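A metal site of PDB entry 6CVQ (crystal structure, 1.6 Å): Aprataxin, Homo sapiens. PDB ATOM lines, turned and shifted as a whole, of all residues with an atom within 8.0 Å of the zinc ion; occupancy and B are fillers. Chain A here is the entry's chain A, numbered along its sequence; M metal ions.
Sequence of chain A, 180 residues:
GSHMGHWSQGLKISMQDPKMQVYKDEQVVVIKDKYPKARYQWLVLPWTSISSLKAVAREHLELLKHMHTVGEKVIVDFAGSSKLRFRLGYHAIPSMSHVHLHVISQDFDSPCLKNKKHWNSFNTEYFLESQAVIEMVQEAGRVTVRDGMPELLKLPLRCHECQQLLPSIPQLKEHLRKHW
Of the 16 residues printed, 4 come within 4 Å of the zinc ion. The nearest printed residue that does not touch the zinc ion is Glu 161 (4.3 Å).
The backbone NH (N) of Glu 161 sits close to the side-chain sulfur (SG) of Cys 159, 3.3 Å away. N of Cys 159 lies within hydrogen-bond range of O of Gln 164 (2.9 Å). The side-chain sulfur of Cys 162 lies close to the backbone NH of Gln 164 (3.7 Å).
The zinc ion is bound by a ring nitrogen (NE2) of His 175 (2.0 Å), a ring nitrogen (NE2) of His 179 (2.1 Å), the side-chain sulfur of Cys 162 (2.2 Å) and the side-chain sulfur of Cys 159 (2.4 Å).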
ATOM      1  N   TRP A 119     -11.789  23.029  27.809  1.00  0.00           N
ATOM      2  CA  TRP A 119     -10.520  23.579  27.361  1.00  0.00           C
ATOM      3  C   TRP A 119     -10.660  25.071  27.048  1.00  0.00           C
ATOM      4  O   TRP A 119      -9.899  25.899  27.560  1.00  0.00           O
ATOM      5  CB  TRP A 119     -10.013  22.821  26.133  1.00  0.00           C
ATOM      6  CG  TRP A 119      -8.741  23.399  25.685  1.00  0.00           C
ATOM      7  CD1 TRP A 119      -8.545  24.195  24.603  1.00  0.00           C
ATOM      8  CD2 TRP A 119      -7.473  23.278  26.330  1.00  0.00           C
ATOM      9  NE1 TRP A 119      -7.230  24.589  24.533  1.00  0.00           N
ATOM     10  CE2 TRP A 119      -6.542  24.033  25.589  1.00  0.00           C
ATOM     11  CE3 TRP A 119      -7.028  22.615  27.486  1.00  0.00           C
ATOM     12  CZ2 TRP A 119      -5.197  24.129  25.952  1.00  0.00           C
ATOM     13  CZ3 TRP A 119      -5.705  22.714  27.839  1.00  0.00           C
ATOM     14  CH2 TRP A 119      -4.803  23.459  27.079  1.00  0.00           C
ATOM     15  N   ARG A 158      -6.352  24.279  20.742  1.00  0.00           N
ATOM     16  CA  ARG A 158      -5.028  24.853  20.531  1.00  0.00           C
ATOM     17  C   ARG A 158      -4.275  24.875  21.848  1.00  0.00           C
ATOM     18  O   ARG A 158      -4.811  25.327  22.866  1.00  0.00           O
ATOM     19  CB  ARG A 158      -5.129  26.274  19.967  1.00  0.00           C
ATOM     20  CG  ARG A 158      -3.787  26.926  19.647  1.00  0.00           C
ATOM     21  CD  ARG A 158      -3.956  28.408  19.316  1.00  0.00           C
ATOM     22  NE  ARG A 158      -4.751  28.617  18.105  1.00  0.00           N
ATOM     23  CZ  ARG A 158      -4.277  28.569  16.870  1.00  0.00           C
ATOM     24  NH1 ARG A 158      -2.994  28.306  16.663  1.00  0.00           N
ATOM     25  NH2 ARG A 158      -5.068  28.774  15.831  1.00  0.00           N
ATOM     26  N   CYS A 159      -3.044  24.394  21.827  1.00  0.00           N
ATOM     27  CA  CYS A 159      -2.208  24.445  23.016  1.00  0.00           C
ATOM     28  C   CYS A 159      -1.956  25.872  23.468  1.00  0.00           C
ATOM     29  O   CYS A 159      -1.708  26.777  22.657  1.00  0.00           O
ATOM     30  CB  CYS A 159      -0.869  23.756  22.747  1.00  0.00           C
ATOM     31  SG  CYS A 159       0.228  23.748  24.171  1.00  0.00           S
ATOM     32  N   HIS A 160      -2.026  26.075  24.779  1.00  0.00           N
ATOM     33  CA  HIS A 160      -1.794  27.381  25.372  1.00  0.00           C
ATOM     34  C   HIS A 160      -0.310  27.721  25.535  1.00  0.00           C
ATOM     35  O   HIS A 160       0.031  28.892  25.757  1.00  0.00           O
ATOM     36  CB  HIS A 160      -2.485  27.447  26.726  1.00  0.00           C
ATOM     37  CG  HIS A 160      -1.932  26.488  27.730  1.00  0.00           C
ATOM     38  ND1 HIS A 160      -1.681  25.151  27.431  1.00  0.00           N
ATOM     39  CD2 HIS A 160      -1.586  26.646  29.035  1.00  0.00           C
ATOM     40  CE1 HIS A 160      -1.217  24.551  28.511  1.00  0.00           C
ATOM     41  NE2 HIS A 160      -1.148  25.435  29.500  1.00  0.00           N
ATOM     42  N   GLU A 161       0.583  26.735  25.422  1.00  0.00           N
ATOM     43  CA  GLU A 161       2.006  26.975  25.599  1.00  0.00           C
ATOM     44  C   GLU A 161       2.701  27.286  24.279  1.00  0.00           C
ATOM     45  O   GLU A 161       3.544  28.195  24.212  1.00  0.00           O
ATOM     46  CB  GLU A 161       2.665  25.761  26.236  1.00  0.00           C
ATOM     47  CG  GLU A 161       2.155  25.426  27.620  1.00  0.00           C
ATOM     48  CD  GLU A 161       2.673  26.388  28.663  1.00  0.00           C
ATOM     49  OE1 GLU A 161       3.750  26.986  28.439  1.00  0.00           O
ATOM     50  OE2 GLU A 161       1.990  26.530  29.716  1.00  0.00           O
ATOM     51  N   CYS A 162       2.373  26.529  23.235  1.00  0.00           N
ATOM     52  CA  CYS A 162       3.088  26.615  21.975  1.00  0.00           C
ATOM     53  C   CYS A 162       2.174  26.867  20.780  1.00  0.00           C
ATOM     54  O   CYS A 162       2.663  26.958  19.654  1.00  0.00           O
ATOM     55  CB  CYS A 162       3.889  25.324  21.725  1.00  0.00           C
ATOM     56  SG  CYS A 162       2.909  23.857  21.341  1.00  0.00           S
ATOM     57  N   GLN A 163       0.854  26.984  20.995  1.00  0.00           N
ATOM     58  CA  GLN A 163      -0.114  27.375  19.973  1.00  0.00           C
ATOM     59  C   GLN A 163      -0.335  26.298  18.905  1.00  0.00           C
ATOM     60  O   GLN A 163      -1.023  26.561  17.916  1.00  0.00           O
ATOM     61  CB  GLN A 163       0.288  28.686  19.285  1.00  0.00           C
ATOM     62  CG  GLN A 163       0.186  29.927  20.188  1.00  0.00           C
ATOM     63  CD  GLN A 163       1.195  29.936  21.327  1.00  0.00           C
ATOM     64  OE1 GLN A 163       2.404  30.003  21.114  1.00  0.00           O
ATOM     65  NE2 GLN A 163       0.683  29.867  22.562  1.00  0.00           N
ATOM     66  N   GLN A 164       0.202  25.095  19.067  1.00  0.00           N
ATOM     67  CA  GLN A 164      -0.074  24.022  18.125  1.00  0.00           C
ATOM     68  C   GLN A 164      -1.549  23.642  18.163  1.00  0.00           C
ATOM     69  O   GLN A 164      -2.173  23.598  19.222  1.00  0.00           O
ATOM     70  CB  GLN A 164       0.802  22.810  18.422  1.00  0.00           C
ATOM     71  CG  GLN A 164       0.721  21.701  17.372  1.00  0.00           C
ATOM     72  CD  GLN A 164       1.714  20.567  17.642  1.00  0.00           C
ATOM     73  OE1 GLN A 164       2.786  20.793  18.215  1.00  0.00           O
ATOM     74  NE2 GLN A 164       1.351  19.352  17.241  1.00  0.00           N
ATOM     75  N   LEU A 165      -2.102  23.342  16.993  1.00  0.00           N
ATOM     76  CA  LEU A 165      -3.475  22.888  16.870  1.00  0.00           C
ATOM     77  C   LEU A 165      -3.515  21.379  17.055  1.00  0.00           C
ATOM     78  O   LEU A 165      -2.693  20.668  16.473  1.00  0.00           O
ATOM     79  CB  LEU A 165      -4.055  23.288  15.513  1.00  0.00           C
ATOM     80  CG  LEU A 165      -4.254  24.792  15.307  1.00  0.00           C
ATOM     81  CD1 LEU A 165      -4.455  25.118  13.822  1.00  0.00           C
ATOM     82  CD2 LEU A 165      -5.432  25.313  16.130  1.00  0.00           C
ATOM     83  N   LEU A 166      -4.455  20.909  17.865  1.00  0.00           N
ATOM     84  CA  LEU A 166      -4.603  19.482  18.157  1.00  0.00           C
ATOM     85  C   LEU A 166      -6.002  19.030  17.758  1.00  0.00           C
ATOM     86  O   LEU A 166      -6.955  19.794  17.896  1.00  0.00           O
ATOM     87  CB  LEU A 166      -4.371  19.173  19.649  1.00  0.00           C
ATOM     88  CG  LEU A 166      -2.919  19.103  20.177  1.00  0.00           C
ATOM     89  CD1 LEU A 166      -2.050  18.128  19.379  1.00  0.00           C
ATOM     90  CD2 LEU A 166      -2.280  20.441  20.202  1.00  0.00           C
ATOM     91  N   LEU A 172      -4.641  16.202  22.637  1.00  0.00           N
ATOM     92  CA  LEU A 172      -4.201  17.387  23.363  1.00  0.00           C
ATOM     93  C   LEU A 172      -3.565  16.996  24.699  1.00  0.00           C
ATOM     94  O   LEU A 172      -2.533  17.537  25.080  1.00  0.00           O
ATOM     95  CB  LEU A 172      -5.367  18.347  23.578  1.00  0.00           C
ATOM     96  CG  LEU A 172      -5.099  19.557  24.467  1.00  0.00           C
ATOM     97  CD1 LEU A 172      -3.990  20.422  23.875  1.00  0.00           C
ATOM     98  CD2 LEU A 172      -6.370  20.374  24.672  1.00  0.00           C
ATOM     99  N   HIS A 175      -0.196  15.705  24.107  1.00  0.00           N
ATOM    100  CA  HIS A 175       0.676  16.816  23.750  1.00  0.00           C
ATOM    101  C   HIS A 175       1.117  17.598  24.974  1.00  0.00           C
ATOM    102  O   HIS A 175       2.285  17.964  25.106  1.00  0.00           O
ATOM    103  CB  HIS A 175      -0.040  17.738  22.757  1.00  0.00           C
ATOM    104  CG  HIS A 175       0.699  19.005  22.482  1.00  0.00           C
ATOM    105  ND1 HIS A 175       1.655  19.121  21.490  1.00  0.00           N
ATOM    106  CD2 HIS A 175       0.614  20.237  23.059  1.00  0.00           C
ATOM    107  CE1 HIS A 175       2.133  20.359  21.474  1.00  0.00           C
ATOM    108  NE2 HIS A 175       1.515  21.050  22.422  1.00  0.00           N
ATOM    109  N   LEU A 176       0.178  17.889  25.878  1.00  0.00           N
ATOM    110  CA  LEU A 176       0.491  18.725  27.033  1.00  0.00           C
ATOM    111  C   LEU A 176       1.622  18.139  27.879  1.00  0.00           C
ATOM    112  O   LEU A 176       2.300  18.888  28.597  1.00  0.00           O
ATOM    113  CB  LEU A 176      -0.767  18.907  27.883  1.00  0.00           C
ATOM    114  CG  LEU A 176      -1.861  19.803  27.300  1.00  0.00           C
ATOM    115  CD1 LEU A 176      -3.107  19.712  28.165  1.00  0.00           C
ATOM    116  CD2 LEU A 176      -1.397  21.244  27.195  1.00  0.00           C
ATOM    117  N   ARG A 177       1.853  16.829  27.816  1.00  0.00           N
ATOM    118  CA  ARG A 177       2.927  16.223  28.601  1.00  0.00           C
ATOM    119  C   ARG A 177       4.278  16.867  28.311  1.00  0.00           C
ATOM    120  O   ARG A 177       5.113  16.980  29.214  1.00  0.00           O
ATOM    121  CB  ARG A 177       2.997  14.723  28.336  1.00  0.00           C
ATOM    122  CG  ARG A 177       1.866  13.918  28.935  1.00  0.00           C
ATOM    123  CD  ARG A 177       2.047  12.426  28.674  1.00  0.00           C
ATOM    124  NE  ARG A 177       1.275  11.618  29.631  1.00  0.00           N
ATOM    125  CZ  ARG A 177       1.757  11.157  30.796  1.00  0.00           C
ATOM    126  NH1 ARG A 177       3.010  11.400  31.157  1.00  0.00           N
ATOM    127  NH2 ARG A 177       0.979  10.439  31.590  1.00  0.00           N
ATOM    128  N   LYS A 178       4.520  17.289  27.073  1.00  0.00           N
ATOM    129  CA  LYS A 178       5.827  17.846  26.742  1.00  0.00           C
ATOM    130  C   LYS A 178       6.105  19.143  27.494  1.00  0.00           C
ATOM    131  O   LYS A 178       7.270  19.553  27.584  1.00  0.00           O
ATOM    132  CB  LYS A 178       5.931  18.078  25.230  1.00  0.00           C
ATOM    133  CG  LYS A 178       5.183  19.293  24.705  1.00  0.00           C
ATOM    134  CD  LYS A 178       5.746  19.763  23.384  1.00  0.00           C
ATOM    135  CE  LYS A 178       5.563  18.740  22.287  1.00  0.00           C
ATOM    136  NZ  LYS A 178       6.048  19.283  20.974  1.00  0.00           N
ATOM    137  N   HIS A 179       5.082  19.802  28.015  1.00  0.00           N
ATOM    138  CA  HIS A 179       5.244  21.094  28.672  1.00  0.00           C
ATOM    139  C   HIS A 179       5.336  20.980  30.184  1.00  0.00           C
ATOM    140  O   HIS A 179       5.315  22.002  30.877  1.00  0.00           O
ATOM    141  CB  HIS A 179       4.100  22.021  28.274  1.00  0.00           C
ATOM    142  CG  HIS A 179       4.033  22.309  26.811  1.00  0.00           C
ATOM    143  ND1 HIS A 179       5.072  22.899  26.129  1.00  0.00           N
ATOM    144  CD2 HIS A 179       3.056  22.092  25.901  1.00  0.00           C
ATOM    145  CE1 HIS A 179       4.733  23.038  24.861  1.00  0.00           C
ATOM    146  NE2 HIS A 179       3.516  22.544  24.687  1.00  0.00           N
HETATM  147 ZN    ZN M   1       2.144  22.817  23.172  1.00  0.00          ZN
